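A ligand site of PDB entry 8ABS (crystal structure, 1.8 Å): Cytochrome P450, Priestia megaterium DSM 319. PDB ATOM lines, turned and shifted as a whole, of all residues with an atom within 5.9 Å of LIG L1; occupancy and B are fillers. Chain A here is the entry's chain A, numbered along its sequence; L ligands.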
ATOM      1  N   TYR A  12     -10.971  18.404 -30.278  1.00  0.00           N
ATOM      2  CA  TYR A  12     -10.207  18.040 -29.086  1.00  0.00           C
ATOM      3  C   TYR A  12     -11.077  18.165 -27.843  1.00  0.00           C
ATOM      4  O   TYR A  12     -11.470  19.275 -27.444  1.00  0.00           O
ATOM      5  CB  TYR A  12      -8.960  18.923 -28.985  1.00  0.00           C
ATOM      6  CG  TYR A  12      -7.959  18.515 -27.921  1.00  0.00           C
ATOM      7  CD1 TYR A  12      -7.804  17.185 -27.541  1.00  0.00           C
ATOM      8  CD2 TYR A  12      -7.158  19.475 -27.307  1.00  0.00           C
ATOM      9  CE1 TYR A  12      -6.888  16.822 -26.576  1.00  0.00           C
ATOM     10  CE2 TYR A  12      -6.244  19.121 -26.344  1.00  0.00           C
ATOM     11  CZ  TYR A  12      -6.106  17.785 -25.977  1.00  0.00           C
ATOM     12  OH  TYR A  12      -5.193  17.430 -25.013  1.00  0.00           O
ATOM     13  N   ASN A  14     -10.489  17.991 -24.778  1.00  0.00           N
ATOM     14  CA  ASN A  14      -9.963  18.711 -23.628  1.00  0.00           C
ATOM     15  C   ASN A  14     -10.333  20.180 -23.664  1.00  0.00           C
ATOM     16  O   ASN A  14     -10.198  20.868 -22.645  1.00  0.00           O
ATOM     17  CB  ASN A  14      -8.449  18.549 -23.546  1.00  0.00           C
ATOM     18  CG  ASN A  14      -7.947  18.476 -22.093  1.00  0.00           C
ATOM     19  OD1 ASN A  14      -8.710  18.166 -21.163  1.00  0.00           O
ATOM     20  ND2 ASN A  14      -6.668  18.786 -21.899  1.00  0.00           N
ATOM     21  N   ARG A  74      -2.084  14.669 -30.574  1.00  0.00           N
ATOM     22  CA  ARG A  74      -3.535  15.008 -30.464  1.00  0.00           C
ATOM     23  C   ARG A  74      -3.871  16.378 -31.056  1.00  0.00           C
ATOM     24  O   ARG A  74      -4.967  16.864 -30.762  1.00  0.00           O
ATOM     25  CB  ARG A  74      -3.951  14.969 -28.991  1.00  0.00           C
ATOM     26  CG  ARG A  74      -3.191  15.893 -28.045  1.00  0.00           C
ATOM     27  CD  ARG A  74      -3.326  15.362 -26.630  1.00  0.00           C
ATOM     28  NE  ARG A  74      -2.693  16.164 -25.594  1.00  0.00           N
ATOM     29  CZ  ARG A  74      -1.392  16.170 -25.306  1.00  0.00           C
ATOM     30  NH1 ARG A  74      -0.534  15.446 -25.999  1.00  0.00           N
ATOM     31  NH2 ARG A  74      -0.960  16.921 -24.316  1.00  0.00           N
ATOM     32  N   LEU A  84       5.363  18.753 -26.986  1.00  0.00           N
ATOM     33  CA  LEU A  84       4.143  18.391 -26.253  1.00  0.00           C
ATOM     34  C   LEU A  84       3.291  17.417 -27.046  1.00  0.00           C
ATOM     35  O   LEU A  84       2.625  16.546 -26.467  1.00  0.00           O
ATOM     36  CB  LEU A  84       3.331  19.655 -25.959  1.00  0.00           C
ATOM     37  CG  LEU A  84       2.019  19.438 -25.225  1.00  0.00           C
ATOM     38  CD1 LEU A  84       2.275  18.890 -23.838  1.00  0.00           C
ATOM     39  CD2 LEU A  84       1.218  20.729 -25.154  1.00  0.00           C
ATOM     40  N   MET A  85       3.314  17.536 -28.370  1.00  0.00           N
ATOM     41  CA  MET A  85       2.446  16.772 -29.255  1.00  0.00           C
ATOM     42  C   MET A  85       3.190  15.710 -30.029  1.00  0.00           C
ATOM     43  O   MET A  85       2.699  15.204 -31.031  1.00  0.00           O
ATOM     44  CB  MET A  85       1.756  17.728 -30.237  1.00  0.00           C
ATOM     45  CG  MET A  85       1.079  18.896 -29.563  1.00  0.00           C
ATOM     46  SD  MET A  85      -0.573  18.418 -29.019  1.00  0.00           S
ATOM     47  CE  MET A  85      -1.078  19.875 -28.091  1.00  0.00           C
ATOM     48  N   VAL A 168      -4.699  28.871 -24.791  1.00  0.00           N
ATOM     49  CA  VAL A 168      -5.246  27.819 -23.926  1.00  0.00           C
ATOM     50  C   VAL A 168      -6.749  27.916 -23.797  1.00  0.00           C
ATOM     51  O   VAL A 168      -7.345  27.125 -23.046  1.00  0.00           O
ATOM     52  CB  VAL A 168      -4.598  27.818 -22.522  1.00  0.00           C
ATOM     53  CG1 VAL A 168      -3.071  27.721 -22.628  1.00  0.00           C
ATOM     54  CG2 VAL A 168      -5.026  29.040 -21.734  1.00  0.00           C
ATOM     55  N   LEU A 237       5.511  26.963 -27.241  1.00  0.00           N
ATOM     56  CA  LEU A 237       5.223  26.076 -26.127  1.00  0.00           C
ATOM     57  C   LEU A 237       5.859  26.587 -24.840  1.00  0.00           C
ATOM     58  O   LEU A 237       5.212  26.653 -23.795  1.00  0.00           O
ATOM     59  CB  LEU A 237       5.719  24.653 -26.434  1.00  0.00           C
ATOM     60  CG  LEU A 237       5.659  23.704 -25.241  1.00  0.00           C
ATOM     61  CD1 LEU A 237       4.259  23.520 -24.717  1.00  0.00           C
ATOM     62  CD2 LEU A 237       6.234  22.363 -25.672  1.00  0.00           C
ATOM     63  N   VAL A 240       4.017  29.802 -23.543  1.00  0.00           N
ATOM     64  CA  VAL A 240       2.676  29.624 -23.015  1.00  0.00           C
ATOM     65  C   VAL A 240       2.702  28.761 -21.764  1.00  0.00           C
ATOM     66  O   VAL A 240       2.107  29.107 -20.750  1.00  0.00           O
ATOM     67  CB  VAL A 240       1.758  29.024 -24.087  1.00  0.00           C
ATOM     68  CG1 VAL A 240       0.418  28.693 -23.478  1.00  0.00           C
ATOM     69  CG2 VAL A 240       1.590  30.003 -25.245  1.00  0.00           C
ATOM     70  N   ALA A 241       3.379  27.607 -21.828  1.00  0.00           N
ATOM     71  CA  ALA A 241       3.501  26.755 -20.651  1.00  0.00           C
ATOM     72  C   ALA A 241       4.260  27.478 -19.537  1.00  0.00           C
ATOM     73  O   ALA A 241       3.936  27.318 -18.352  1.00  0.00           O
ATOM     74  CB  ALA A 241       4.204  25.451 -21.006  1.00  0.00           C
ATOM     75  N   GLU A 244       1.377  30.768 -18.451  1.00  0.00           N
ATOM     76  CA  GLU A 244      -0.050  30.655 -18.144  1.00  0.00           C
ATOM     77  C   GLU A 244      -0.293  29.793 -16.898  1.00  0.00           C
ATOM     78  O   GLU A 244      -1.133  30.128 -16.060  1.00  0.00           O
ATOM     79  CB  GLU A 244      -0.791  30.079 -19.347  1.00  0.00           C
ATOM     80  CG  GLU A 244      -2.308  30.269 -19.320  1.00  0.00           C
ATOM     81  CD  GLU A 244      -3.023  29.202 -18.471  1.00  0.00           C
ATOM     82  OE1 GLU A 244      -2.450  28.125 -18.239  1.00  0.00           O
ATOM     83  OE2 GLU A 244      -4.173  29.487 -18.042  1.00  0.00           O
ATOM     84  N   THR A 245       0.440  28.703 -16.800  1.00  0.00           N
ATOM     85  CA  THR A 245       0.291  27.781 -15.675  1.00  0.00           C
ATOM     86  C   THR A 245       0.836  28.392 -14.397  1.00  0.00           C
ATOM     87  O   THR A 245       0.184  28.373 -13.346  1.00  0.00           O
ATOM     88  CB  THR A 245       1.027  26.482 -15.990  1.00  0.00           C
ATOM     89  OG1 THR A 245       2.384  26.793 -16.324  1.00  0.00           O
ATOM     90  CG2 THR A 245       0.407  25.783 -17.181  1.00  0.00           C
ATOM     91  N   ILE A 288      -3.319  22.864 -14.337  1.00  0.00           N
ATOM     92  CA  ILE A 288      -3.774  22.025 -15.439  1.00  0.00           C
ATOM     93  C   ILE A 288      -4.629  20.919 -14.833  1.00  0.00           C
ATOM     94  O   ILE A 288      -4.134  20.103 -14.016  1.00  0.00           O
ATOM     95  CB  ILE A 288      -2.618  21.452 -16.257  1.00  0.00           C
ATOM     96  CG1 ILE A 288      -1.806  22.586 -16.932  1.00  0.00           C
ATOM     97  CG2 ILE A 288      -3.151  20.456 -17.295  1.00  0.00           C
ATOM     98  CD1 ILE A 288      -2.616  23.474 -17.880  1.00  0.00           C
ATOM     99  N   ALA A 290      -6.542  18.582 -16.646  1.00  0.00           N
ATOM    100  CA  ALA A 290      -6.745  17.413 -17.494  1.00  0.00           C
ATOM    101  C   ALA A 290      -5.699  17.401 -18.593  1.00  0.00           C
ATOM    102  O   ALA A 290      -5.351  18.455 -19.150  1.00  0.00           O
ATOM    103  CB  ALA A 290      -8.152  17.428 -18.094  1.00  0.00           C
ATOM    104  N   ILE A 291      -5.228  16.198 -18.921  1.00  0.00           N
ATOM    105  CA  ILE A 291      -4.189  15.963 -19.913  1.00  0.00           C
ATOM    106  C   ILE A 291      -4.740  14.985 -20.936  1.00  0.00           C
ATOM    107  O   ILE A 291      -5.172  13.883 -20.589  1.00  0.00           O
ATOM    108  CB  ILE A 291      -2.923  15.373 -19.261  1.00  0.00           C
ATOM    109  CG1 ILE A 291      -2.373  16.306 -18.189  1.00  0.00           C
ATOM    110  CG2 ILE A 291      -1.887  15.080 -20.338  1.00  0.00           C
ATOM    111  CD1 ILE A 291      -1.369  15.629 -17.287  1.00  0.00           C
ATOM    112  N   GLY A 292      -4.678  15.375 -22.212  1.00  0.00           N
ATOM    113  CA  GLY A 292      -5.246  14.564 -23.279  1.00  0.00           C
ATOM    114  C   GLY A 292      -4.253  13.585 -23.890  1.00  0.00           C
ATOM    115  O   GLY A 292      -3.043  13.819 -23.906  1.00  0.00           O
ATOM    116  N   ARG A 293      -4.796  12.482 -24.392  1.00  0.00           N
ATOM    117  CA  ARG A 293      -4.055  11.503 -25.167  1.00  0.00           C
ATOM    118  C   ARG A 293      -4.970  10.945 -26.242  1.00  0.00           C
ATOM    119  O   ARG A 293      -6.199  11.128 -26.218  1.00  0.00           O
ATOM    120  CB  ARG A 293      -3.522  10.352 -24.278  1.00  0.00           C
ATOM    121  CG  ARG A 293      -2.456  10.761 -23.267  1.00  0.00           C
ATOM    122  CD  ARG A 293      -1.149  11.079 -23.960  1.00  0.00           C
ATOM    123  NE  ARG A 293      -0.037  11.296 -23.029  1.00  0.00           N
ATOM    124  CZ  ARG A 293       0.313  12.478 -22.560  1.00  0.00           C
ATOM    125  NH1 ARG A 293      -0.399  13.569 -22.807  1.00  0.00           N
ATOM    126  NH2 ARG A 293       1.419  12.576 -21.821  1.00  0.00           N
ATOM    127  N   PHE A 389      -9.654  22.701 -19.261  1.00  0.00           N
ATOM    128  CA  PHE A 389      -8.478  21.965 -18.775  1.00  0.00           C
ATOM    129  C   PHE A 389      -7.577  22.825 -17.926  1.00  0.00           C
ATOM    130  O   PHE A 389      -6.567  22.344 -17.412  1.00  0.00           O
ATOM    131  CB  PHE A 389      -7.704  21.344 -19.945  1.00  0.00           C
ATOM    132  CG  PHE A 389      -6.876  22.325 -20.742  1.00  0.00           C
ATOM    133  CD1 PHE A 389      -5.544  22.535 -20.418  1.00  0.00           C
ATOM    134  CD2 PHE A 389      -7.401  22.958 -21.836  1.00  0.00           C
ATOM    135  CE1 PHE A 389      -4.764  23.388 -21.152  1.00  0.00           C
ATOM    136  CE2 PHE A 389      -6.629  23.840 -22.575  1.00  0.00           C
ATOM    137  CZ  PHE A 389      -5.302  24.043 -22.222  1.00  0.00           C
HETATM  138  C1  LIG L   1       0.467  24.495 -21.418  1.00  0.00           C
HETATM  139  C2  LIG L   1       0.716  23.631 -20.266  1.00  0.00           C
HETATM  140  C3  LIG L   1       1.120  22.202 -20.700  1.00  0.00           C
HETATM  141  C4  LIG L   1       2.247  22.126 -21.692  1.00  0.00           C
HETATM  142  C5  LIG L   1      -0.060  21.556 -21.465  1.00  0.00           C
HETATM  143  C6  LIG L   1      -0.397  20.225 -20.827  1.00  0.00           C
HETATM  144  C7  LIG L   1      -0.903  20.621 -19.490  1.00  0.00           C
HETATM  145  C8  LIG L   1      -1.373  19.353 -21.752  1.00  0.00           C
HETATM  146  C9  LIG L   1      -2.679  20.026 -21.864  1.00  0.00           C
HETATM  147  C10 LIG L   1      -3.501  19.018 -22.719  1.00  0.00           C
HETATM  148  O1  LIG L   1      -3.246  17.797 -22.586  1.00  0.00           O
HETATM  149  O2  LIG L   1      -4.354  19.494 -23.495  1.00  0.00           O
HETATM  150 FE1  LG2 L   2       4.874  22.460 -17.854  1.00  0.00          FE
HETATM  151  C1  LG2 L   2       4.692  19.707 -19.917  1.00  0.00           C
HETATM  152  C2  LG2 L   2       2.027  21.481 -16.280  1.00  0.00           C
HETATM  153  C3  LG2 L   2       5.112  25.205 -15.794  1.00  0.00           C
HETATM  154  C4  LG2 L   2       7.227  23.847 -19.946  1.00  0.00           C
HETATM  155  N1  LG2 L   2       3.582  20.900 -18.095  1.00  0.00           N
HETATM  156  C5  LG2 L   2       3.761  19.794 -18.922  1.00  0.00           C
HETATM  157  C6  LG2 L   2       2.742  18.816 -18.597  1.00  0.00           C
HETATM  158  C7  LG2 L   2       2.025  19.329 -17.586  1.00  0.00           C
HETATM  159  C8  LG2 L   2       2.516  20.639 -17.261  1.00  0.00           C
HETATM  160  C9  LG2 L   2       0.823  18.677 -16.865  1.00  0.00           C
HETATM  161  C10 LG2 L   2       2.552  17.413 -19.241  1.00  0.00           C
HETATM  162  C11 LG2 L   2       1.567  17.421 -20.398  1.00  0.00           C
HETATM  163  C12 LG2 L   2       1.431  16.088 -21.090  1.00  0.00           C
HETATM  164  O1  LG2 L   2       1.781  15.024 -20.507  1.00  0.00           O
HETATM  165  O2  LG2 L   2       0.951  16.069 -22.259  1.00  0.00           O
HETATM  166  N2  LG2 L   2       3.759  23.234 -16.376  1.00  0.00           N
HETATM  167  C13 LG2 L   2       2.644  22.628 -15.817  1.00  0.00           C
HETATM  168  C14 LG2 L   2       2.265  23.389 -14.622  1.00  0.00           C
HETATM  169  C15 LG2 L   2       3.119  24.402 -14.503  1.00  0.00           C
HETATM  170  C16 LG2 L   2       4.075  24.326 -15.596  1.00  0.00           C
HETATM  171  C17 LG2 L   2       1.085  23.014 -13.673  1.00  0.00           C
HETATM  172  C18 LG2 L   2       3.207  25.515 -13.441  1.00  0.00           C
HETATM  173  C19 LG2 L   2       2.729  25.386 -12.211  1.00  0.00           C
HETATM  174  N3  LG2 L   2       5.918  24.252 -17.886  1.00  0.00           N
HETATM  175  C20 LG2 L   2       5.998  25.157 -16.859  1.00  0.00           C
HETATM  176  C21 LG2 L   2       7.123  26.046 -17.082  1.00  0.00           C
HETATM  177  C22 LG2 L   2       7.684  25.662 -18.253  1.00  0.00           C
HETATM  178  C23 LG2 L   2       6.949  24.517 -18.761  1.00  0.00           C
HETATM  179  C24 LG2 L   2       7.570  27.181 -16.136  1.00  0.00           C
HETATM  180  C25 LG2 L   2       8.925  26.198 -18.980  1.00  0.00           C
HETATM  181  C26 LG2 L   2       9.798  27.035 -18.399  1.00  0.00           C
HETATM  182  N4  LG2 L   2       5.780  21.875 -19.611  1.00  0.00           N
HETATM  183  C27 LG2 L   2       6.723  22.620 -20.312  1.00  0.00           C
HETATM  184  C28 LG2 L   2       7.058  21.887 -21.518  1.00  0.00           C
HETATM  185  C29 LG2 L   2       6.357  20.746 -21.522  1.00  0.00           C
HETATM  186  C30 LG2 L   2       5.549  20.713 -20.320  1.00  0.00           C
HETATM  187  C31 LG2 L   2       8.074  22.377 -22.582  1.00  0.00           C
HETATM  188  C32 LG2 L   2       6.370  19.638 -22.590  1.00  0.00           C
HETATM  189  C33 LG2 L   2       7.259  18.482 -22.144  1.00  0.00           C
HETATM  190  C34 LG2 L   2       7.165  17.348 -23.139  1.00  0.00           C
HETATM  191  O3  LG2 L   2       8.127  16.519 -23.154  1.00  0.00           O
HETATM  192  O4  LG2 L   2       6.171  17.277 -23.896  1.00  0.00           O
HETATM  193  C1  LG3 L   3       0.579  26.543 -32.753  1.00  0.00           C
HETATM  194  C2  LG3 L   3       1.577  27.645 -33.059  1.00  0.00           C
HETATM  195  C3  LG3 L   3       2.914  27.074 -33.423  1.00  0.00           C
HETATM  196  O1  LG3 L   3       3.616  27.521 -34.318  1.00  0.00           O
HETATM  197  C4  LG3 L   3       3.283  25.917 -32.624  1.00  0.00           C
HETATM  198  C5  LG3 L   3       2.525  25.474 -31.621  1.00  0.00           C
HETATM  199  C6  LG3 L   3       3.172  24.584 -30.614  1.00  0.00           C
HETATM  200  C7  LG3 L   3       2.686  25.015 -29.229  1.00  0.00           C
HETATM  201  C8  LG3 L   3       1.161  24.918 -29.156  1.00  0.00           C
HETATM  202  C9  LG3 L   3       0.501  25.835 -30.222  1.00  0.00           C
HETATM  203  C10 LG3 L   3       1.006  25.515 -31.663  1.00  0.00           C
HETATM  204  C11 LG3 L   3      -1.026  25.819 -30.045  1.00  0.00           C
HETATM  205  C12 LG3 L   3      -1.488  26.129 -28.611  1.00  0.00           C
HETATM  206  C13 LG3 L   3      -0.833  25.193 -27.583  1.00  0.00           C
HETATM  207  C14 LG3 L   3       0.689  25.280 -27.767  1.00  0.00           C
HETATM  208  C15 LG3 L   3       1.243  24.517 -26.556  1.00  0.00           C
HETATM  209  C16 LG3 L   3       0.303  24.984 -25.418  1.00  0.00           C
HETATM  210  C17 LG3 L   3      -0.916  25.618 -26.118  1.00  0.00           C
HETATM  211  O2  LG3 L   3      -2.159  25.246 -25.533  1.00  0.00           O
HETATM  212  C18 LG3 L   3      -1.358  23.753 -27.757  1.00  0.00           C
HETATM  213  C19 LG3 L   3       0.460  24.189 -32.176  1.00  0.00           C
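An oxygen (O2) of LIG L1 sits at hydrogen-bond distance from the side-chain hydroxyl (OH) of Tyr 12. NH2 of Arg 293 lies within salt-bridge range of O1 of LG2 L2, at 2.8 Å. An oxygen (O1) of LIG L1 is in salt-bridge range of the guanidinium group (NH2) of Arg 74 (3.0 Å). N of Gly 292 is in hydrogen-bond range of O1 of LIG L1. An oxygen (O2) of LG2 L2 is in salt-bridge range of the guanidinium group (NH2) of Arg 74, 2.9 Å away. An oxygen (O2) of LIG L1 sits at hydrogen-bond distance from the side-chain amide nitrogen (ND2) of Asn 14 (2.9 Å).
Leu 84 touches LIG L1 (CD2 to C4, 3.9 Å). Leu 237 touches LIG L1. Ala 241 touches LIG L1. CG2 of Thr 245 touches C2 of LIG L1 (3.8 Å). Ile 288 touches LIG L1. Ile 291 touches LIG L1 (CA to O1, 3.4 Å). Of the 17 residues printed, 10 come within 4 Å of LIG L1.
The backbone carbonyl oxygen of Ala 241 sits at hydrogen-bond distance from the side-chain hydroxyl of Thr 245 (2.6 Å). The backbone carbonyl oxygen of Gly 292 lies within hydrogen-bond range of the guanidinium group of Arg 74, 2.9 Å away. The backbone carbonyl oxygen (O) of Ala 290 sits at hydrogen-bond distance from the side-chain amide nitrogen (ND2) of Asn 14 (3.1 Å). The side-chain hydroxyl (OH) of Tyr 12 lies within hydrogen-bond range of the guanidinium group (NE) of Arg 74. O of Leu 84 lies within hydrogen-bond range of NH1 of Arg 74 (3.4 Å).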
